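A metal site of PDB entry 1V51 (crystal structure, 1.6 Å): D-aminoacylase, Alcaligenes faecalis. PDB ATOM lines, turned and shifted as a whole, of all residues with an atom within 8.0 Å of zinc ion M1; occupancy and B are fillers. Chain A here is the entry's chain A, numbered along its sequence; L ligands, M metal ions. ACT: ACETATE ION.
The nearest printed residue that does not touch zinc ion M1 is Tyr 205 (4.3 Å).
Zinc ion M1 is bound by ND1 of His 233, NE2 of His 263, O of the ligand, SG of Cys 109 and OXT of the ligand.
O of Thr 201 sits at hydrogen-bond distance from N of His 233, 2.9 Å away.
ND1 of His 263 is in hydrogen-bond range of OE2 of Glu 237, at 3.1 Å.
O of His 263 lies within hydrogen-bond range of NZ of Lys 265, at 3.1 Å.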
ATOM      1  N   HIS A  80     -32.088  10.418 -15.646  1.00  0.00           N
ATOM      2  CA  HIS A  80     -31.080  10.583 -14.609  1.00  0.00           C
ATOM      3  C   HIS A  80     -30.824   9.289 -13.864  1.00  0.00           C
ATOM      4  O   HIS A  80     -31.602   8.913 -12.980  1.00  0.00           O
ATOM      5  CB  HIS A  80     -31.538  11.649 -13.600  1.00  0.00           C
ATOM      6  CG  HIS A  80     -30.488  11.988 -12.585  1.00  0.00           C
ATOM      7  ND1 HIS A  80     -29.622  13.050 -12.735  1.00  0.00           N
ATOM      8  CD2 HIS A  80     -30.146  11.385 -11.419  1.00  0.00           C
ATOM      9  CE1 HIS A  80     -28.783  13.076 -11.709  1.00  0.00           C
ATOM     10  NE2 HIS A  80     -29.076  12.077 -10.900  1.00  0.00           N
ATOM     11  N   HIS A  82     -27.728   6.321 -12.207  1.00  0.00           N
ATOM     12  CA  HIS A  82     -26.392   6.022 -11.730  1.00  0.00           C
ATOM     13  C   HIS A  82     -26.194   4.530 -12.019  1.00  0.00           C
ATOM     14  O   HIS A  82     -25.747   3.752 -11.164  1.00  0.00           O
ATOM     15  CB  HIS A  82     -26.254   6.356 -10.250  1.00  0.00           C
ATOM     16  CG  HIS A  82     -26.312   7.832  -9.989  1.00  0.00           C
ATOM     17  ND1 HIS A  82     -25.327   8.697 -10.399  1.00  0.00           N
ATOM     18  CD2 HIS A  82     -27.297   8.596  -9.460  1.00  0.00           C
ATOM     19  CE1 HIS A  82     -25.693   9.941 -10.136  1.00  0.00           C
ATOM     20  NE2 HIS A  82     -26.899   9.899  -9.565  1.00  0.00           N
ATOM     21  N   ASN A 108     -23.996  10.726 -14.138  1.00  0.00           N
ATOM     22  CA  ASN A 108     -24.587  11.953 -13.634  1.00  0.00           C
ATOM     23  C   ASN A 108     -23.932  12.522 -12.372  1.00  0.00           C
ATOM     24  O   ASN A 108     -23.245  11.819 -11.637  1.00  0.00           O
ATOM     25  CB  ASN A 108     -26.065  11.673 -13.379  1.00  0.00           C
ATOM     26  CG  ASN A 108     -26.846  11.595 -14.656  1.00  0.00           C
ATOM     27  OD1 ASN A 108     -27.228  10.507 -15.127  1.00  0.00           O
ATOM     28  ND2 ASN A 108     -27.065  12.740 -15.262  1.00  0.00           N
ATOM     29  N   CYS A 109     -24.156  13.822 -12.137  1.00  0.00           N
ATOM     30  CA  CYS A 109     -23.671  14.532 -10.964  1.00  0.00           C
ATOM     31  C   CYS A 109     -22.164  14.513 -10.816  1.00  0.00           C
ATOM     32  O   CYS A 109     -21.655  14.566  -9.684  1.00  0.00           O
ATOM     33  CB  CYS A 109     -24.302  13.934  -9.701  1.00  0.00           C
ATOM     34  SG  CYS A 109     -26.110  13.816  -9.867  1.00  0.00           S
ATOM     35  N   GLY A 110     -21.469  14.472 -11.955  1.00  0.00           N
ATOM     36  CA  GLY A 110     -20.017  14.435 -11.968  1.00  0.00           C
ATOM     37  C   GLY A 110     -19.455  13.064 -11.662  1.00  0.00           C
ATOM     38  O   GLY A 110     -18.235  12.894 -11.628  1.00  0.00           O
ATOM     39  N   ILE A 111     -20.346  12.090 -11.479  1.00  0.00           N
ATOM     40  CA  ILE A 111     -19.979  10.706 -11.135  1.00  0.00           C
ATOM     41  C   ILE A 111     -20.076   9.709 -12.289  1.00  0.00           C
ATOM     42  O   ILE A 111     -21.181   9.321 -12.669  1.00  0.00           O
ATOM     43  CB  ILE A 111     -20.902  10.148 -10.022  1.00  0.00           C
ATOM     44  CG1 ILE A 111     -20.962  11.109  -8.824  1.00  0.00           C
ATOM     45  CG2 ILE A 111     -20.394   8.776  -9.574  1.00  0.00           C
ATOM     46  CD1 ILE A 111     -22.126  10.762  -7.877  1.00  0.00           C
ATOM     47  N   PRO A 124     -18.840  10.785  -3.501  1.00  0.00           N
ATOM     48  CA  PRO A 124     -19.869   9.781  -3.772  1.00  0.00           C
ATOM     49  C   PRO A 124     -19.600   8.818  -4.932  1.00  0.00           C
ATOM     50  O   PRO A 124     -20.515   8.135  -5.396  1.00  0.00           O
ATOM     51  CB  PRO A 124     -21.100  10.644  -4.030  1.00  0.00           C
ATOM     52  CG  PRO A 124     -20.504  11.790  -4.820  1.00  0.00           C
ATOM     53  CD  PRO A 124     -19.251  12.101  -4.018  1.00  0.00           C
ATOM     54  N   LEU A 127     -20.818   5.226  -4.900  1.00  0.00           N
ATOM     55  CA  LEU A 127     -22.201   4.830  -5.174  1.00  0.00           C
ATOM     56  C   LEU A 127     -22.288   3.881  -6.373  1.00  0.00           C
ATOM     57  O   LEU A 127     -23.310   3.219  -6.570  1.00  0.00           O
ATOM     58  CB  LEU A 127     -23.074   6.052  -5.423  1.00  0.00           C
ATOM     59  CG  LEU A 127     -23.423   6.897  -4.197  1.00  0.00           C
ATOM     60  CD1 LEU A 127     -24.224   8.104  -4.626  1.00  0.00           C
ATOM     61  CD2 LEU A 127     -24.214   6.051  -3.186  1.00  0.00           C
ATOM     62  N   THR A 201     -21.411  17.520 -13.858  1.00  0.00           N
ATOM     63  CA  THR A 201     -20.675  17.998 -12.689  1.00  0.00           C
ATOM     64  C   THR A 201     -21.549  17.870 -11.443  1.00  0.00           C
ATOM     65  O   THR A 201     -22.780  17.716 -11.539  1.00  0.00           O
ATOM     66  CB  THR A 201     -20.288  19.476 -12.800  1.00  0.00           C
ATOM     67  OG1 THR A 201     -21.493  20.250 -12.859  1.00  0.00           O
ATOM     68  CG2 THR A 201     -19.439  19.727 -14.044  1.00  0.00           C
ATOM     69  N   GLY A 202     -20.896  17.931 -10.298  1.00  0.00           N
ATOM     70  CA  GLY A 202     -21.575  17.853  -9.015  1.00  0.00           C
ATOM     71  C   GLY A 202     -20.695  18.538  -7.980  1.00  0.00           C
ATOM     72  O   GLY A 202     -20.159  17.877  -7.082  1.00  0.00           O
ATOM     73  N   PHE A 204     -21.417  20.148  -5.529  1.00  0.00           N
ATOM     74  CA  PHE A 204     -21.983  20.051  -4.185  1.00  0.00           C
ATOM     75  C   PHE A 204     -21.159  19.029  -3.380  1.00  0.00           C
ATOM     76  O   PHE A 204     -20.994  19.151  -2.145  1.00  0.00           O
ATOM     77  CB  PHE A 204     -23.432  19.538  -4.291  1.00  0.00           C
ATOM     78  CG  PHE A 204     -24.011  19.051  -2.984  1.00  0.00           C
ATOM     79  CD1 PHE A 204     -24.460  19.965  -2.037  1.00  0.00           C
ATOM     80  CD2 PHE A 204     -24.128  17.697  -2.715  1.00  0.00           C
ATOM     81  CE1 PHE A 204     -25.026  19.528  -0.843  1.00  0.00           C
ATOM     82  CE2 PHE A 204     -24.695  17.251  -1.522  1.00  0.00           C
ATOM     83  CZ  PHE A 204     -25.147  18.176  -0.587  1.00  0.00           C
ATOM     84  N   TYR A 205     -20.610  18.032  -4.073  1.00  0.00           N
ATOM     85  CA  TYR A 205     -19.843  16.958  -3.412  1.00  0.00           C
ATOM     86  C   TYR A 205     -18.365  17.255  -3.133  1.00  0.00           C
ATOM     87  O   TYR A 205     -17.735  18.045  -3.825  1.00  0.00           O
ATOM     88  CB  TYR A 205     -19.973  15.667  -4.219  1.00  0.00           C
ATOM     89  CG  TYR A 205     -21.402  15.120  -4.204  1.00  0.00           C
ATOM     90  CD1 TYR A 205     -21.942  14.595  -3.042  1.00  0.00           C
ATOM     91  CD2 TYR A 205     -22.208  15.163  -5.352  1.00  0.00           C
ATOM     92  CE1 TYR A 205     -23.259  14.117  -2.999  1.00  0.00           C
ATOM     93  CE2 TYR A 205     -23.528  14.697  -5.321  1.00  0.00           C
ATOM     94  CZ  TYR A 205     -24.042  14.168  -4.145  1.00  0.00           C
ATOM     95  OH  TYR A 205     -25.324  13.668  -4.109  1.00  0.00           O
ATOM     96  N   THR A 232     -25.876  18.931 -14.665  1.00  0.00           N
ATOM     97  CA  THR A 232     -25.360  19.308 -13.358  1.00  0.00           C
ATOM     98  C   THR A 232     -26.204  19.058 -12.122  1.00  0.00           C
ATOM     99  O   THR A 232     -27.413  19.252 -12.124  1.00  0.00           O
ATOM    100  CB  THR A 232     -25.001  20.821 -13.364  1.00  0.00           C
ATOM    101  OG1 THR A 232     -24.448  21.200 -12.081  1.00  0.00           O
ATOM    102  CG2 THR A 232     -26.246  21.680 -13.596  1.00  0.00           C
ATOM    103  N   HIS A 233     -25.516  18.614 -11.074  1.00  0.00           N
ATOM    104  CA  HIS A 233     -26.095  18.511  -9.749  1.00  0.00           C
ATOM    105  C   HIS A 233     -25.593  19.873  -9.265  1.00  0.00           C
ATOM    106  O   HIS A 233     -24.397  20.047  -9.035  1.00  0.00           O
ATOM    107  CB  HIS A 233     -25.442  17.389  -8.939  1.00  0.00           C
ATOM    108  CG  HIS A 233     -25.895  17.339  -7.512  1.00  0.00           C
ATOM    109  ND1 HIS A 233     -26.240  16.155  -6.897  1.00  0.00           N
ATOM    110  CD2 HIS A 233     -26.046  18.315  -6.584  1.00  0.00           C
ATOM    111  CE1 HIS A 233     -26.586  16.402  -5.635  1.00  0.00           C
ATOM    112  NE2 HIS A 233     -26.464  17.700  -5.423  1.00  0.00           N
ATOM    113  N   MET A 234     -26.487  20.844  -9.131  1.00  0.00           N
ATOM    114  CA  MET A 234     -26.061  22.202  -8.761  1.00  0.00           C
ATOM    115  C   MET A 234     -25.285  22.299  -7.471  1.00  0.00           C
ATOM    116  O   MET A 234     -25.436  21.475  -6.569  1.00  0.00           O
ATOM    117  CB  MET A 234     -27.261  23.149  -8.816  1.00  0.00           C
ATOM    118  CG  MET A 234     -27.843  23.225 -10.238  1.00  0.00           C
ATOM    119  SD  MET A 234     -29.107  24.489 -10.391  1.00  0.00           S
ATOM    120  CE  MET A 234     -30.334  23.879  -9.202  1.00  0.00           C
ATOM    121  N   GLU A 237     -28.695  23.298  -3.436  1.00  0.00           N
ATOM    122  CA  GLU A 237     -30.103  23.163  -3.792  1.00  0.00           C
ATOM    123  C   GLU A 237     -31.014  23.638  -2.646  1.00  0.00           C
ATOM    124  O   GLU A 237     -32.176  23.242  -2.563  1.00  0.00           O
ATOM    125  CB  GLU A 237     -30.416  21.712  -4.145  1.00  0.00           C
ATOM    126  CG  GLU A 237     -29.654  21.192  -5.370  1.00  0.00           C
ATOM    127  CD  GLU A 237     -30.113  19.792  -5.777  1.00  0.00           C
ATOM    128  OE1 GLU A 237     -29.933  18.859  -4.968  1.00  0.00           O
ATOM    129  OE2 GLU A 237     -30.660  19.618  -6.900  1.00  0.00           O
ATOM    130  N   SER A 262     -30.102  18.647 -13.007  1.00  0.00           N
ATOM    131  CA  SER A 262     -30.508  17.353 -12.442  1.00  0.00           C
ATOM    132  C   SER A 262     -31.353  17.436 -11.185  1.00  0.00           C
ATOM    133  O   SER A 262     -31.142  18.308 -10.343  1.00  0.00           O
ATOM    134  CB  SER A 262     -29.275  16.521 -12.074  1.00  0.00           C
ATOM    135  OG  SER A 262     -28.438  16.312 -13.191  1.00  0.00           O
ATOM    136  N   HIS A 263     -32.260  16.453 -11.060  1.00  0.00           N
ATOM    137  CA  HIS A 263     -33.130  16.299  -9.895  1.00  0.00           C
ATOM    138  C   HIS A 263     -33.495  17.613  -9.229  1.00  0.00           C
ATOM    139  O   HIS A 263     -33.137  17.847  -8.077  1.00  0.00           O
ATOM    140  CB  HIS A 263     -32.505  15.302  -8.865  1.00  0.00           C
ATOM    141  CG  HIS A 263     -31.053  15.531  -8.540  1.00  0.00           C
ATOM    142  ND1 HIS A 263     -30.556  16.717  -8.037  1.00  0.00           N
ATOM    143  CD2 HIS A 263     -29.994  14.683  -8.575  1.00  0.00           C
ATOM    144  CE1 HIS A 263     -29.259  16.595  -7.791  1.00  0.00           C
ATOM    145  NE2 HIS A 263     -28.892  15.359  -8.098  1.00  0.00           N
ATOM    146  N   LYS A 265     -35.119  20.423  -7.173  1.00  0.00           N
ATOM    147  CA  LYS A 265     -35.818  20.418  -5.891  1.00  0.00           C
ATOM    148  C   LYS A 265     -35.419  21.650  -5.090  1.00  0.00           C
ATOM    149  O   LYS A 265     -34.500  22.391  -5.462  1.00  0.00           O
ATOM    150  CB  LYS A 265     -35.356  19.207  -5.076  1.00  0.00           C
ATOM    151  CG  LYS A 265     -33.846  19.341  -4.696  1.00  0.00           C
ATOM    152  CD  LYS A 265     -33.366  18.263  -3.724  1.00  0.00           C
ATOM    153  CE  LYS A 265     -33.189  16.942  -4.384  1.00  0.00           C
ATOM    154  NZ  LYS A 265     -32.039  16.941  -5.374  1.00  0.00           N
ATOM    155  N   TYR A 296     -37.373  13.480  -9.881  1.00  0.00           N
ATOM    156  CA  TYR A 296     -37.942  12.185  -9.524  1.00  0.00           C
ATOM    157  C   TYR A 296     -39.184  12.535  -8.677  1.00  0.00           C
ATOM    158  O   TYR A 296     -39.230  13.552  -7.973  1.00  0.00           O
ATOM    159  CB  TYR A 296     -36.925  11.301  -8.777  1.00  0.00           C
ATOM    160  CG  TYR A 296     -36.232  11.958  -7.620  1.00  0.00           C
ATOM    161  CD1 TYR A 296     -36.850  12.055  -6.371  1.00  0.00           C
ATOM    162  CD2 TYR A 296     -34.947  12.490  -7.778  1.00  0.00           C
ATOM    163  CE1 TYR A 296     -36.194  12.666  -5.288  1.00  0.00           C
ATOM    164  CE2 TYR A 296     -34.281  13.103  -6.712  1.00  0.00           C
ATOM    165  CZ  TYR A 296     -34.918  13.184  -5.476  1.00  0.00           C
ATOM    166  OH  TYR A 296     -34.256  13.790  -4.426  1.00  0.00           O
ATOM    167  N   SER A 302     -31.586  10.789  -1.891  1.00  0.00           N
ATOM    168  CA  SER A 302     -30.703   9.708  -1.467  1.00  0.00           C
ATOM    169  C   SER A 302     -29.344   9.877  -2.130  1.00  0.00           C
ATOM    170  O   SER A 302     -29.254  10.215  -3.307  1.00  0.00           O
ATOM    171  CB  SER A 302     -31.305   8.342  -1.834  1.00  0.00           C
ATOM    172  OG  SER A 302     -30.510   7.274  -1.330  1.00  0.00           O
ATOM    173  N   THR A 303     -28.273   9.666  -1.352  1.00  0.00           N
ATOM    174  CA  THR A 303     -26.906   9.786  -1.855  1.00  0.00           C
ATOM    175  C   THR A 303     -25.973   9.358  -0.723  1.00  0.00           C
ATOM    176  O   THR A 303     -26.414   8.678   0.185  1.00  0.00           O
ATOM    177  CB  THR A 303     -26.584  11.241  -2.319  1.00  0.00           C
ATOM    178  OG1 THR A 303     -25.260  11.258  -2.861  1.00  0.00           O
ATOM    179  CG2 THR A 303     -26.693  12.244  -1.166  1.00  0.00           C
ATOM    180  N   ASP A 379     -33.125   8.567 -10.638  1.00  0.00           N
ATOM    181  CA  ASP A 379     -32.029   8.781  -9.683  1.00  0.00           C
ATOM    182  C   ASP A 379     -31.861   7.505  -8.835  1.00  0.00           C
ATOM    183  O   ASP A 379     -31.447   7.560  -7.676  1.00  0.00           O
ATOM    184  CB  ASP A 379     -32.278   9.992  -8.778  1.00  0.00           C
ATOM    185  CG  ASP A 379     -30.980  10.635  -8.311  1.00  0.00           C
ATOM    186  OD1 ASP A 379     -29.908  10.092  -8.633  1.00  0.00           O
ATOM    187  OD2 ASP A 379     -31.041  11.679  -7.635  1.00  0.00           O
ATOM    188  N   LEU A 381     -30.268   4.339  -7.145  1.00  0.00           N
ATOM    189  CA  LEU A 381     -28.885   4.002  -6.705  1.00  0.00           C
ATOM    190  C   LEU A 381     -29.001   2.489  -6.572  1.00  0.00           C
ATOM    191  O   LEU A 381     -29.284   1.949  -5.487  1.00  0.00           O
ATOM    192  CB  LEU A 381     -28.568   4.696  -5.375  1.00  0.00           C
ATOM    193  CG  LEU A 381     -28.746   6.230  -5.383  1.00  0.00           C
ATOM    194  CD1 LEU A 381     -28.324   6.826  -4.064  1.00  0.00           C
ATOM    195  CD2 LEU A 381     -27.888   6.823  -6.493  1.00  0.00           C
ATOM    196  N   ARG A 390     -37.462   4.851  -5.434  1.00  0.00           N
ATOM    197  CA  ARG A 390     -37.481   5.479  -6.761  1.00  0.00           C
ATOM    198  C   ARG A 390     -36.777   4.578  -7.770  1.00  0.00           C
ATOM    199  O   ARG A 390     -37.036   4.633  -8.987  1.00  0.00           O
ATOM    200  CB  ARG A 390     -36.808   6.865  -6.709  1.00  0.00           C
ATOM    201  CG  ARG A 390     -35.323   6.842  -6.354  1.00  0.00           C
ATOM    202  CD  ARG A 390     -34.864   8.242  -5.948  1.00  0.00           C
ATOM    203  NE  ARG A 390     -33.411   8.332  -5.815  1.00  0.00           N
ATOM    204  CZ  ARG A 390     -32.780   9.398  -5.322  1.00  0.00           C
ATOM    205  NH1 ARG A 390     -33.473  10.444  -4.901  1.00  0.00           N
ATOM    206  NH2 ARG A 390     -31.453   9.428  -5.315  1.00  0.00           N
HETATM  207  C   ACT L   1     -27.188  12.245  -6.743  1.00  0.00           C
HETATM  208  O   ACT L   1     -26.560  13.244  -6.330  1.00  0.00           O
HETATM  209  OXT ACT L   1     -28.074  12.325  -7.608  1.00  0.00           O
HETATM  210  CH3 ACT L   1     -26.951  10.907  -6.085  1.00  0.00           C
HETATM  211 ZN    ZN M   1     -27.016  14.561  -7.905  1.00  0.00          ZN
HETATM  212 ZN    ZN M   2     -28.406  11.229  -9.187  1.00  0.00          ZN
